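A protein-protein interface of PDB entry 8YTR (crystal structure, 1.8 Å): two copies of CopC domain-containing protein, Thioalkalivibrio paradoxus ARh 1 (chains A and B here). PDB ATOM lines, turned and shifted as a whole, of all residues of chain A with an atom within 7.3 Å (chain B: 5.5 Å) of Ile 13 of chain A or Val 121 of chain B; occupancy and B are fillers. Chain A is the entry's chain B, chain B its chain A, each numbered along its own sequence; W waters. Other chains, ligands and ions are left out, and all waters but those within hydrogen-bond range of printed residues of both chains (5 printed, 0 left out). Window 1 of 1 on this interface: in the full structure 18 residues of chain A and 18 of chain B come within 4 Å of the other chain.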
ATOM      1  N   PRO A   9      10.196  32.513 -21.616  1.00  0.00           N
ATOM      2  CA  PRO A   9       9.447  31.898 -22.714  1.00  0.00           C
ATOM      3  C   PRO A   9       7.963  32.074 -22.575  1.00  0.00           C
ATOM      4  O   PRO A   9       7.454  32.190 -21.475  1.00  0.00           O
ATOM      5  CB  PRO A   9       9.835  30.407 -22.619  1.00  0.00           C
ATOM      6  CG  PRO A   9      10.946  30.357 -21.646  1.00  0.00           C
ATOM      7  CD  PRO A   9      10.830  31.517 -20.753  1.00  0.00           C
ATOM      8  N   PRO A  10       7.227  32.095 -23.706  1.00  0.00           N
ATOM      9  CA  PRO A  10       5.782  32.205 -23.685  1.00  0.00           C
ATOM     10  C   PRO A  10       5.175  30.880 -23.247  1.00  0.00           C
ATOM     11  O   PRO A  10       5.885  29.887 -23.036  1.00  0.00           O
ATOM     12  CB  PRO A  10       5.432  32.551 -25.143  1.00  0.00           C
ATOM     13  CG  PRO A  10       6.528  31.876 -25.907  1.00  0.00           C
ATOM     14  CD  PRO A  10       7.776  32.030 -25.079  1.00  0.00           C
ATOM     15  N   GLU A  11       3.863  30.858 -23.152  1.00  0.00           N
ATOM     16  CA  GLU A  11       3.186  29.612 -22.837  1.00  0.00           C
ATOM     17  C   GLU A  11       3.182  28.753 -24.112  1.00  0.00           C
ATOM     18  O   GLU A  11       2.230  28.787 -24.869  1.00  0.00           O
ATOM     19  CB  GLU A  11       1.773  29.857 -22.299  1.00  0.00           C
ATOM     20  CG  GLU A  11       1.130  28.507 -22.028  1.00  0.00           C
ATOM     21  CD  GLU A  11      -0.147  28.378 -21.268  1.00  0.00           C
ATOM     22  OE1 GLU A  11      -1.232  28.904 -21.658  1.00  0.00           O
ATOM     23  OE2 GLU A  11       0.047  27.648 -20.267  1.00  0.00           O
ATOM     24  N   ALA A  12       4.248  27.964 -24.287  1.00  0.00           N
ATOM     25  CA  ALA A  12       4.474  27.192 -25.497  1.00  0.00           C
ATOM     26  C   ALA A  12       5.515  26.129 -25.196  1.00  0.00           C
ATOM     27  O   ALA A  12       6.078  26.105 -24.112  1.00  0.00           O
ATOM     28  CB  ALA A  12       4.968  28.115 -26.582  1.00  0.00           C
ATOM     29  N   ILE A  13       5.679  25.227 -26.147  1.00  0.00           N
ATOM     30  CA  ILE A  13       6.773  24.287 -26.207  1.00  0.00           C
ATOM     31  C   ILE A  13       7.908  24.953 -26.963  1.00  0.00           C
ATOM     32  O   ILE A  13       7.763  25.239 -28.156  1.00  0.00           O
ATOM     33  CB  ILE A  13       6.333  22.991 -26.884  1.00  0.00           C
ATOM     34  CG1 ILE A  13       5.073  22.418 -26.226  1.00  0.00           C
ATOM     35  CG2 ILE A  13       7.473  21.970 -26.896  1.00  0.00           C
ATOM     36  CD1 ILE A  13       4.349  21.417 -27.095  1.00  0.00           C
ATOM     37  N   VAL A  14       9.012  25.183 -26.259  1.00  0.00           N
ATOM     38  CA  VAL A  14      10.179  25.823 -26.854  1.00  0.00           C
ATOM     39  C   VAL A  14      11.392  24.910 -26.722  1.00  0.00           C
ATOM     40  O   VAL A  14      11.459  23.999 -25.905  1.00  0.00           O
ATOM     41  CB  VAL A  14      10.485  27.173 -26.180  1.00  0.00           C
ATOM     42  CG1 VAL A  14       9.319  28.140 -26.402  1.00  0.00           C
ATOM     43  CG2 VAL A  14      10.854  26.984 -24.712  1.00  0.00           C
ATOM     44  N   ASP A  15      12.327  25.140 -27.619  1.00  0.00           N
ATOM     45  CA  ASP A  15      13.585  24.428 -27.621  1.00  0.00           C
ATOM     46  C   ASP A  15      14.544  25.176 -26.696  1.00  0.00           C
ATOM     47  O   ASP A  15      14.675  24.826 -25.522  1.00  0.00           O
ATOM     48  CB  ASP A  15      14.116  24.305 -29.042  1.00  0.00           C
ATOM     49  CG  ASP A  15      14.954  23.049 -29.212  1.00  0.00           C
ATOM     50  OD1 ASP A  15      15.902  22.877 -28.383  1.00  0.00           O
ATOM     51  OD2 ASP A  15      14.597  22.248 -30.122  1.00  0.00           O
ATOM     52  N   LEU A  44       5.071  15.393 -14.653  1.00  0.00           N
ATOM     53  CA  LEU A  44       4.044  14.975 -15.595  1.00  0.00           C
ATOM     54  C   LEU A  44       3.426  13.642 -15.172  1.00  0.00           C
ATOM     55  O   LEU A  44       4.166  12.763 -14.803  1.00  0.00           O
ATOM     56  CB  LEU A  44       4.688  14.842 -16.959  1.00  0.00           C
ATOM     57  CG  LEU A  44       5.231  16.143 -17.558  1.00  0.00           C
ATOM     58  CD1 LEU A  44       5.725  15.850 -18.961  1.00  0.00           C
ATOM     59  CD2 LEU A  44       4.201  17.235 -17.559  1.00  0.00           C
ATOM     60  N   ILE A  49       1.105  14.732 -21.102  1.00  0.00           N
ATOM     61  CA  ILE A  49      -0.007  15.646 -21.308  1.00  0.00           C
ATOM     62  C   ILE A  49      -0.102  15.946 -22.794  1.00  0.00           C
ATOM     63  O   ILE A  49       0.870  15.812 -23.528  1.00  0.00           O
ATOM     64  CB  ILE A  49       0.176  16.929 -20.488  1.00  0.00           C
ATOM     65  CG1 ILE A  49       1.428  17.684 -20.849  1.00  0.00           C
ATOM     66  CG2 ILE A  49       0.178  16.626 -18.997  1.00  0.00           C
ATOM     67  CD1 ILE A  49       1.517  19.066 -20.214  1.00  0.00           C
ATOM     68  N   ARG A  50      -1.285  16.388 -23.197  1.00  0.00           N
ATOM     69  CA  ARG A  50      -1.653  16.517 -24.587  1.00  0.00           C
ATOM     70  C   ARG A  50      -1.843  17.966 -25.012  1.00  0.00           C
ATOM     71  O   ARG A  50      -1.823  18.215 -26.203  1.00  0.00           O
ATOM     72  CB  ARG A  50      -2.851  15.623 -24.850  1.00  0.00           C
ATOM     73  CG  ARG A  50      -2.354  14.191 -25.020  1.00  0.00           C
ATOM     74  CD  ARG A  50      -3.403  13.092 -24.943  1.00  0.00           C
ATOM     75  NE  ARG A  50      -2.763  11.765 -25.025  1.00  0.00           N
ATOM     76  CZ  ARG A  50      -1.922  11.156 -24.160  1.00  0.00           C
ATOM     77  NH1 ARG A  50      -1.539  11.729 -23.030  1.00  0.00           N
ATOM     78  NH2 ARG A  50      -1.449   9.954 -24.443  1.00  0.00           N
ATOM     79  N   ASN A  51      -1.994  18.906 -24.083  1.00  0.00           N
ATOM     80  CA  ASN A  51      -2.260  20.288 -24.446  1.00  0.00           C
ATOM     81  C   ASN A  51      -1.847  21.220 -23.316  1.00  0.00           C
ATOM     82  O   ASN A  51      -1.590  20.768 -22.222  1.00  0.00           O
ATOM     83  CB  ASN A  51      -3.702  20.497 -24.882  1.00  0.00           C
ATOM     84  CG  ASN A  51      -4.721  20.128 -23.831  1.00  0.00           C
ATOM     85  OD1 ASN A  51      -4.627  20.524 -22.678  1.00  0.00           O
ATOM     86  ND2 ASN A  51      -5.722  19.370 -24.210  1.00  0.00           N
ATOM     87  N   LEU A  52      -1.850  22.514 -23.607  1.00  0.00           N
ATOM     88  CA  LEU A  52      -1.493  23.547 -22.646  1.00  0.00           C
ATOM     89  C   LEU A  52      -2.514  23.717 -21.526  1.00  0.00           C
ATOM     90  O   LEU A  52      -2.167  24.193 -20.456  1.00  0.00           O
ATOM     91  CB  LEU A  52      -1.435  24.879 -23.388  1.00  0.00           C
ATOM     92  CG  LEU A  52      -0.355  25.034 -24.442  1.00  0.00           C
ATOM     93  CD1 LEU A  52      -0.509  26.486 -24.970  1.00  0.00           C
ATOM     94  CD2 LEU A  52       1.048  24.672 -23.982  1.00  0.00           C
ATOM     95  N   LEU A  55      -1.365  21.456 -18.999  1.00  0.00           N
ATOM     96  CA  LEU A  55      -0.203  22.040 -18.359  1.00  0.00           C
ATOM     97  C   LEU A  55      -0.603  23.036 -17.280  1.00  0.00           C
ATOM     98  O   LEU A  55      -0.030  23.051 -16.177  1.00  0.00           O
ATOM     99  CB  LEU A  55       0.680  22.695 -19.436  1.00  0.00           C
ATOM    100  CG  LEU A  55       1.934  23.401 -18.929  1.00  0.00           C
ATOM    101  CD1 LEU A  55       2.935  22.375 -18.483  1.00  0.00           C
ATOM    102  CD2 LEU A  55       2.539  24.330 -19.994  1.00  0.00           C
ATOM    103  N   ALA A 119       3.112  29.039 -17.353  1.00  0.00           N
ATOM    104  CA  ALA A 119       3.746  27.741 -17.551  1.00  0.00           C
ATOM    105  C   ALA A 119       4.295  27.601 -18.964  1.00  0.00           C
ATOM    106  O   ALA A 119       3.834  28.267 -19.850  1.00  0.00           O
ATOM    107  CB  ALA A 119       2.720  26.678 -17.218  1.00  0.00           C
ATOM    108  N   PHE A 120       5.322  26.781 -19.161  1.00  0.00           N
ATOM    109  CA  PHE A 120       5.842  26.512 -20.488  1.00  0.00           C
ATOM    110  C   PHE A 120       6.552  25.161 -20.478  1.00  0.00           C
ATOM    111  O   PHE A 120       6.743  24.562 -19.429  1.00  0.00           O
ATOM    112  CB  PHE A 120       6.815  27.612 -20.917  1.00  0.00           C
ATOM    113  CG  PHE A 120       8.039  27.762 -20.022  1.00  0.00           C
ATOM    114  CD1 PHE A 120       9.204  27.032 -20.254  1.00  0.00           C
ATOM    115  CD2 PHE A 120       8.016  28.582 -18.910  1.00  0.00           C
ATOM    116  CE1 PHE A 120      10.314  27.197 -19.415  1.00  0.00           C
ATOM    117  CE2 PHE A 120       9.108  28.749 -18.106  1.00  0.00           C
ATOM    118  CZ  PHE A 120      10.257  28.043 -18.347  1.00  0.00           C
ATOM    119  N   VAL A 121       6.917  24.674 -21.671  1.00  0.00           N
ATOM    120  CA  VAL A 121       7.621  23.409 -21.776  1.00  0.00           C
ATOM    121  C   VAL A 121       8.957  23.691 -22.449  1.00  0.00           C
ATOM    122  O   VAL A 121       8.951  24.193 -23.571  1.00  0.00           O
ATOM    123  CB  VAL A 121       6.850  22.332 -22.574  1.00  0.00           C
ATOM    124  CG1 VAL A 121       7.675  21.030 -22.697  1.00  0.00           C
ATOM    125  CG2 VAL A 121       5.483  22.069 -21.994  1.00  0.00           C
ATOM    126  N   HIS A 122      10.042  23.346 -21.745  1.00  0.00           N
ATOM    127  CA  HIS A 122      11.398  23.467 -22.246  1.00  0.00           C
ATOM    128  C   HIS A 122      11.781  22.127 -22.830  1.00  0.00           C
ATOM    129  O   HIS A 122      12.178  21.243 -22.088  1.00  0.00           O
ATOM    130  CB  HIS A 122      12.345  23.828 -21.094  1.00  0.00           C
ATOM    131  CG  HIS A 122      13.765  24.067 -21.472  1.00  0.00           C
ATOM    132  ND1 HIS A 122      14.874  23.855 -20.686  1.00  0.00           N
ATOM    133  CD2 HIS A 122      14.214  24.564 -22.621  1.00  0.00           C
ATOM    134  CE1 HIS A 122      15.956  24.212 -21.379  1.00  0.00           C
ATOM    135  NE2 HIS A 122      15.588  24.620 -22.556  1.00  0.00           N
ATOM    136  N   ALA A 123      11.670  21.976 -24.150  1.00  0.00           N
ATOM    137  CA  ALA A 123      12.029  20.718 -24.792  1.00  0.00           C
ATOM    138  C   ALA A 123      13.388  20.883 -25.472  1.00  0.00           C
ATOM    139  O   ALA A 123      13.540  20.670 -26.649  1.00  0.00           O
ATOM    140  CB  ALA A 123      10.980  20.343 -25.782  1.00  0.00           C
ATOM    141  N   GLY A 124      14.320  21.512 -24.792  1.00  0.00           N
ATOM    142  CA  GLY A 124      15.709  21.532 -25.187  1.00  0.00           C
ATOM    143  C   GLY A 124      16.533  21.368 -23.918  1.00  0.00           C
ATOM    144  O   GLY A 124      16.007  21.496 -22.793  1.00  0.00           O
ATOM    145  N   ALA B  12       2.285  12.898 -27.186  1.00  0.00           N
ATOM    146  CA  ALA B  12       2.131  13.602 -25.915  1.00  0.00           C
ATOM    147  C   ALA B  12       3.444  14.279 -25.565  1.00  0.00           C
ATOM    148  O   ALA B  12       4.449  14.047 -26.212  1.00  0.00           O
ATOM    149  CB  ALA B  12       1.690  12.663 -24.793  1.00  0.00           C
ATOM    150  N   ILE B  13       3.384  15.192 -24.604  1.00  0.00           N
ATOM    151  CA  ILE B  13       4.559  15.710 -23.927  1.00  0.00           C
ATOM    152  C   ILE B  13       4.815  14.776 -22.771  1.00  0.00           C
ATOM    153  O   ILE B  13       4.006  14.703 -21.842  1.00  0.00           O
ATOM    154  CB  ILE B  13       4.325  17.156 -23.441  1.00  0.00           C
ATOM    155  CG1 ILE B  13       3.882  18.065 -24.587  1.00  0.00           C
ATOM    156  CG2 ILE B  13       5.537  17.705 -22.696  1.00  0.00           C
ATOM    157  CD1 ILE B  13       3.108  19.287 -24.091  1.00  0.00           C
ATOM    158  N   VAL B  14       5.960  14.103 -22.831  1.00  0.00           N
ATOM    159  CA  VAL B  14       6.344  13.142 -21.814  1.00  0.00           C
ATOM    160  C   VAL B  14       7.693  13.548 -21.240  1.00  0.00           C
ATOM    161  O   VAL B  14       8.468  14.297 -21.865  1.00  0.00           O
ATOM    162  CB  VAL B  14       6.418  11.736 -22.437  1.00  0.00           C
ATOM    163  CG1 VAL B  14       5.054  11.338 -23.017  1.00  0.00           C
ATOM    164  CG2 VAL B  14       7.515  11.637 -23.484  1.00  0.00           C
ATOM    165  N   ASP B  15       7.957  13.026 -20.054  1.00  0.00           N
ATOM    166  CA  ASP B  15       9.208  13.227 -19.362  1.00  0.00           C
ATOM    167  C   ASP B  15      10.194  12.135 -19.812  1.00  0.00           C
ATOM    168  O   ASP B  15      11.028  12.363 -20.676  1.00  0.00           O
ATOM    169  CB  ASP B  15       8.951  13.315 -17.867  1.00  0.00           C
ATOM    170  CG  ASP B  15       9.990  14.141 -17.132  1.00  0.00           C
ATOM    171  OD1 ASP B  15      11.199  13.887 -17.362  1.00  0.00           O
ATOM    172  OD2 ASP B  15       9.571  15.005 -16.323  1.00  0.00           O
ATOM    173  N   LEU B  44      11.944  23.471 -33.966  1.00  0.00           N
ATOM    174  CA  LEU B  44      10.771  24.298 -33.686  1.00  0.00           C
ATOM    175  C   LEU B  44      10.958  25.707 -34.227  1.00  0.00           C
ATOM    176  O   LEU B  44      12.065  26.224 -34.156  1.00  0.00           O
ATOM    177  CB  LEU B  44      10.574  24.322 -32.173  1.00  0.00           C
ATOM    178  CG  LEU B  44      10.383  22.940 -31.532  1.00  0.00           C
ATOM    179  CD1 LEU B  44      10.273  22.995 -30.016  1.00  0.00           C
ATOM    180  CD2 LEU B  44       9.158  22.311 -32.115  1.00  0.00           C
ATOM    181  N   ASN B  47      10.025  31.047 -30.877  1.00  0.00           N
ATOM    182  CA  ASN B  47       8.789  31.258 -30.104  1.00  0.00           C
ATOM    183  C   ASN B  47       7.931  29.979 -29.976  1.00  0.00           C
ATOM    184  O   ASN B  47       6.908  30.007 -29.304  1.00  0.00           O
ATOM    185  CB  ASN B  47       7.895  32.403 -30.610  1.00  0.00           C
ATOM    186  CG  ASN B  47       8.576  33.752 -30.518  1.00  0.00           C
ATOM    187  OD1 ASN B  47       8.948  34.166 -29.411  1.00  0.00           O
ATOM    188  ND2 ASN B  47       8.692  34.480 -31.629  1.00  0.00           N
ATOM    189  N   GLY B  48       8.296  28.860 -30.612  1.00  0.00           N
ATOM    190  CA  GLY B  48       7.854  27.531 -30.205  1.00  0.00           C
ATOM    191  C   GLY B  48       6.512  27.123 -30.819  1.00  0.00           C
ATOM    192  O   GLY B  48       5.984  27.804 -31.699  1.00  0.00           O
ATOM    193  N   ILE B  49       5.938  26.032 -30.306  1.00  0.00           N
ATOM    194  CA  ILE B  49       4.618  25.607 -30.759  1.00  0.00           C
ATOM    195  C   ILE B  49       3.672  25.480 -29.571  1.00  0.00           C
ATOM    196  O   ILE B  49       4.131  25.370 -28.442  1.00  0.00           O
ATOM    197  CB  ILE B  49       4.699  24.290 -31.529  1.00  0.00           C
ATOM    198  CG1 ILE B  49       5.217  23.152 -30.668  1.00  0.00           C
ATOM    199  CG2 ILE B  49       5.508  24.488 -32.804  1.00  0.00           C
ATOM    200  CD1 ILE B  49       5.090  21.781 -31.312  1.00  0.00           C
ATOM    201  N   ARG B  50       2.380  25.562 -29.843  1.00  0.00           N
ATOM    202  CA  ARG B  50       1.373  25.683 -28.801  1.00  0.00           C
ATOM    203  C   ARG B  50       0.444  24.471 -28.728  1.00  0.00           C
ATOM    204  O   ARG B  50      -0.283  24.365 -27.744  1.00  0.00           O
ATOM    205  CB  ARG B  50       0.573  26.975 -28.959  1.00  0.00           C
ATOM    206  CG  ARG B  50       1.437  28.167 -28.547  1.00  0.00           C
ATOM    207  CD  ARG B  50       1.055  29.526 -29.135  1.00  0.00           C
ATOM    208  NE  ARG B  50       1.957  30.560 -28.580  1.00  0.00           N
ATOM    209  CZ  ARG B  50       3.267  30.774 -28.859  1.00  0.00           C
ATOM    210  NH1 ARG B  50       3.935  29.993 -29.682  1.00  0.00           N
ATOM    211  NH2 ARG B  50       3.924  31.787 -28.323  1.00  0.00           N
ATOM    212  N   ASN B  51       0.444  23.589 -29.737  1.00  0.00           N
ATOM    213  CA  ASN B  51      -0.438  22.427 -29.712  1.00  0.00           C
ATOM    214  C   ASN B  51       0.168  21.333 -30.579  1.00  0.00           C
ATOM    215  O   ASN B  51       1.076  21.558 -31.373  1.00  0.00           O
ATOM    216  CB  ASN B  51      -1.874  22.785 -30.109  1.00  0.00           C
ATOM    217  CG  ASN B  51      -1.977  23.426 -31.474  1.00  0.00           C
ATOM    218  OD1 ASN B  51      -1.465  22.888 -32.468  1.00  0.00           O
ATOM    219  ND2 ASN B  51      -2.546  24.619 -31.547  1.00  0.00           N
ATOM    220  N   LEU B  52      -0.393  20.147 -30.411  1.00  0.00           N
ATOM    221  CA  LEU B  52      -0.016  18.971 -31.157  1.00  0.00           C
ATOM    222  C   LEU B  52      -0.398  19.025 -32.627  1.00  0.00           C
ATOM    223  O   LEU B  52       0.246  18.346 -33.429  1.00  0.00           O
ATOM    224  CB  LEU B  52      -0.655  17.761 -30.486  1.00  0.00           C
ATOM    225  CG  LEU B  52      -0.133  17.436 -29.094  1.00  0.00           C
ATOM    226  CD1 LEU B  52      -0.789  16.129 -28.658  1.00  0.00           C
ATOM    227  CD2 LEU B  52       1.386  17.368 -28.992  1.00  0.00           C
ATOM    228  N   LEU B  55       2.642  20.409 -34.040  1.00  0.00           N
ATOM    229  CA  LEU B  55       3.663  19.385 -34.015  1.00  0.00           C
ATOM    230  C   LEU B  55       3.497  18.460 -35.231  1.00  0.00           C
ATOM    231  O   LEU B  55       4.474  18.143 -35.908  1.00  0.00           O
ATOM    232  CB  LEU B  55       3.566  18.603 -32.705  1.00  0.00           C
ATOM    233  CG  LEU B  55       4.549  17.432 -32.530  1.00  0.00           C
ATOM    234  CD1 LEU B  55       5.997  17.803 -32.422  1.00  0.00           C
ATOM    235  CD2 LEU B  55       4.204  16.520 -31.331  1.00  0.00           C
ATOM    236  N   GLY B  98      13.556  17.131 -26.750  1.00  0.00           N
ATOM    237  CA  GLY B  98      13.201  17.761 -28.010  1.00  0.00           C
ATOM    238  C   GLY B  98      11.876  17.234 -28.518  1.00  0.00           C
ATOM    239  O   GLY B  98      11.271  16.354 -27.898  1.00  0.00           O
ATOM    240  N   ALA B  99      11.457  17.810 -29.639  1.00  0.00           N
ATOM    241  CA  ALA B  99      10.289  17.312 -30.344  1.00  0.00           C
ATOM    242  C   ALA B  99      10.772  16.297 -31.370  1.00  0.00           C
ATOM    243  O   ALA B  99      11.808  16.488 -32.042  1.00  0.00           O
ATOM    244  CB  ALA B  99       9.525  18.444 -30.984  1.00  0.00           C
ATOM    245  N   TYR B 100      10.015  15.191 -31.506  1.00  0.00           N
ATOM    246  CA  TYR B 100      10.433  14.116 -32.397  1.00  0.00           C
ATOM    247  C   TYR B 100       9.317  13.670 -33.322  1.00  0.00           C
ATOM    248  O   TYR B 100       8.163  13.695 -32.929  1.00  0.00           O
ATOM    249  CB  TYR B 100      10.894  12.911 -31.568  1.00  0.00           C
ATOM    250  CG  TYR B 100      12.234  13.128 -30.939  1.00  0.00           C
ATOM    251  CD1 TYR B 100      13.405  12.888 -31.654  1.00  0.00           C
ATOM    252  CD2 TYR B 100      12.322  13.718 -29.696  1.00  0.00           C
ATOM    253  CE1 TYR B 100      14.635  13.120 -31.074  1.00  0.00           C
ATOM    254  CE2 TYR B 100      13.554  13.935 -29.102  1.00  0.00           C
ATOM    255  CZ  TYR B 100      14.707  13.710 -29.826  1.00  0.00           C
ATOM    256  OH  TYR B 100      15.919  13.997 -29.288  1.00  0.00           O
ATOM    257  N   ALA B 119       4.447  11.586 -33.724  1.00  0.00           N
ATOM    258  CA  ALA B 119       5.264  12.636 -33.136  1.00  0.00           C
ATOM    259  C   ALA B 119       5.055  12.720 -31.640  1.00  0.00           C
ATOM    260  O   ALA B 119       4.005  12.346 -31.137  1.00  0.00           O
ATOM    261  CB  ALA B 119       4.921  13.926 -33.795  1.00  0.00           C
ATOM    262  N   PHE B 120       6.081  13.188 -30.915  1.00  0.00           N
ATOM    263  CA  PHE B 120       5.919  13.361 -29.482  1.00  0.00           C
ATOM    264  C   PHE B 120       6.933  14.375 -29.013  1.00  0.00           C
ATOM    265  O   PHE B 120       7.800  14.777 -29.779  1.00  0.00           O
ATOM    266  CB  PHE B 120       6.074  12.045 -28.718  1.00  0.00           C
ATOM    267  CG  PHE B 120       7.434  11.383 -28.900  1.00  0.00           C
ATOM    268  CD1 PHE B 120       8.489  11.672 -28.043  1.00  0.00           C
ATOM    269  CD2 PHE B 120       7.641  10.475 -29.932  1.00  0.00           C
ATOM    270  CE1 PHE B 120       9.720  11.062 -28.211  1.00  0.00           C
ATOM    271  CE2 PHE B 120       8.894   9.896 -30.123  1.00  0.00           C
ATOM    272  CZ  PHE B 120       9.924  10.177 -29.251  1.00  0.00           C
ATOM    273  N   VAL B 121       6.776  14.856 -27.760  1.00  0.00           N
ATOM    274  CA  VAL B 121       7.726  15.817 -27.218  1.00  0.00           C
ATOM    275  C   VAL B 121       8.365  15.189 -25.989  1.00  0.00           C
ATOM    276  O   VAL B 121       7.641  14.828 -25.066  1.00  0.00           O
ATOM    277  CB  VAL B 121       7.064  17.155 -26.852  1.00  0.00           C
ATOM    278  CG1 VAL B 121       8.041  18.107 -26.159  1.00  0.00           C
ATOM    279  CG2 VAL B 121       6.458  17.811 -28.094  1.00  0.00           C
ATOM    280  N   HIS B 122       9.702  15.095 -26.041  1.00  0.00           N
ATOM    281  CA  HIS B 122      10.498  14.541 -24.987  1.00  0.00           C
ATOM    282  C   HIS B 122      10.955  15.693 -24.091  1.00  0.00           C
ATOM    283  O   HIS B 122      11.832  16.420 -24.474  1.00  0.00           O
ATOM    284  CB  HIS B 122      11.698  13.822 -25.591  1.00  0.00           C
ATOM    285  CG  HIS B 122      12.513  13.108 -24.587  1.00  0.00           C
ATOM    286  ND1 HIS B 122      13.867  12.864 -24.677  1.00  0.00           N
ATOM    287  CD2 HIS B 122      12.094  12.568 -23.433  1.00  0.00           C
ATOM    288  CE1 HIS B 122      14.224  12.169 -23.599  1.00  0.00           C
ATOM    289  NE2 HIS B 122      13.172  11.978 -22.821  1.00  0.00           N
ATOM    290  N   ALA B 123      10.288  15.919 -22.973  1.00  0.00           N
ATOM    291  CA  ALA B 123      10.668  17.008 -22.057  1.00  0.00           C
ATOM    292  C   ALA B 123      11.591  16.571 -20.917  1.00  0.00           C
ATOM    293  O   ALA B 123      11.896  17.348 -20.037  1.00  0.00           O
ATOM    294  CB  ALA B 123       9.400  17.643 -21.510  1.00  0.00           C
HETATM  295  O   HOH W   1      -2.234  22.924 -26.439  1.00  0.00           O
HETATM  296  O   HOH W   2      -2.354  20.201 -28.212  1.00  0.00           O
HETATM  297  O   HOH W   3       7.631  14.213 -14.743  1.00  0.00           O
HETATM  298  O   HOH W   4      13.001  19.805 -30.903  1.00  0.00           O
HETATM  299  O   HOH W   5      14.179  23.253 -32.315  1.00  0.00           O
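N of Ile 13 of chain B lies within hydrogen-bond range of O of Ile 49 of chain A (2.8 Å). The backbone carbonyl oxygen (O) of Ile 49 of chain B lies within hydrogen-bond range of the backbone NH (N) of Ile 13 of chain A, at 2.8 Å.
The backbone carbonyl oxygen (O) of Val 121 of chain B lies within hydrogen-bond range of the backbone NH (N) of Val 14 of chain B (2.9 Å). The backbone carbonyl oxygen (O) of Ala 12 of chain A sits at hydrogen-bond distance from the backbone NH (N) of Val 121 of chain A, at 3.0 Å. The backbone carbonyl oxygen of Asp 15 of chain A is in hydrogen-bond range of the backbone NH of Gly 124 of chain A (3.4 Å).
Among the printed residues, pairs that only touch across the chains: Pro 10 of chain A with Asn 47 of chain B, Pro 10 of chain A with Arg 50 of chain B, Glu 11 of chain A with Arg 50 of chain B, Ala 12 of chain A with Asn 47 of chain B, Ala 12 of chain A with Ile 49 of chain B, Ala 12 of chain A with Arg 50 of chain B, Ile 13 of chain A with Ile 13 of chain B, Ile 13 of chain A with Leu 44 of chain B, Ile 13 of chain A with Gly 48 of chain B, Ile 13 of chain A with Val 121 of chain B, Val 14 of chain A with Leu 44 of chain B, Asp 15 of chain A with Leu 44 of chain B, Leu 44 of chain A with Ile 13 of chain B, Leu 44 of chain A with Val 14 of chain B, Leu 44 of chain A with Asp 15 of chain B, Ile 49 of chain A with Ala 12 of chain B, Arg 50 of chain A with Ala 12 of chain B, Arg 50 of chain A with Leu 52 of chain B, Leu 52 of chain A with Arg 50 of chain B, Val 121 of chain A with Ile 13 of chain B, Val 121 of chain A with Ala 123 of chain B, Ala 123 of chain A with Gly 98 of chain B and Ala 123 of chain A with Val 121 of chain B.
Val 121 of chain B touches just these residues of chain A: Ile 13 and Ala 123. Printed residues of chain B within 4 Å of Ile 49 of chain A: Ala 12 and Ile 13. Of the printed residues of chain B, Val 14 of chain A touches Leu 44. Printed residues of chain A within 4 Å of Leu 52 of chain B: Arg 50. Phe 120 of chain A touches none of the printed residues of chain B. Asn 51 of chain A touches none of the printed residues of chain B.
Of the 20 printed residues of chain B, 13 touch a printed residue of chain A. Hydrophobic or aromatic side chains of chain B within 4 Å of the printed part of chain A: Ala 12, Ile 13, Leu 44, Ile 49, Leu 52, Val 121 and Ala 123. Of the 19 printed residues of chain A, 12 touch a printed residue of chain B. Printed residues of chain A that touch a printed residue of chain B: Pro 10, Glu 11, Ala 12, Ile 13, Val 14, Asp 15, Leu 44, Ile 49, Arg 50, Leu 52, Val 121 and Ala 123. Hydrophobic or aromatic side chains of chain A that line the printed part of chain B: Pro 10, Ala 12, Ile 13, Leu 44, Ile 49, Leu 52, Val 121 and Ala 123. Among the printed residues, no Asp or Glu carboxylate lies within 4 Å of a Lys or Arg side-chain nitrogen of the other chain.
Ala 12 of chain A touches Arg 50 of chain B, and with the chains exchanged Arg 50 of chain A touches Ala 12 of chain B. Ile 13 of chain A touches its own counterpart, Ile 13 of chain B. Ile 13 of chain A touches Leu 44 of chain B, and with the chains exchanged Leu 44 of chain A touches Ile 13 of chain B. Positions printed for both chains: 12, 13, 14, 15, 44, 49, 50, 51, 52, 55, 119, 120, 121, 122 and 123.
Water W5 lies within hydrogen-bond range of the side-chain carboxylate of Asp 15 of chain A (2.4 Å) and the backbone NH of Leu 44 of chain B (2.8 Å). Water W3 bridges OD2 of Asp 15 of chain B and N of Leu 44 of chain A. Water W1 lies within hydrogen-bond range of O of Arg 50 of chain B and N of Leu 52 of chain A. Water W4 lies within hydrogen-bond range of N of Ala 99 of chain B (2.8 Å) and OD2 of Asp 15 of chain A (3.0 Å).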
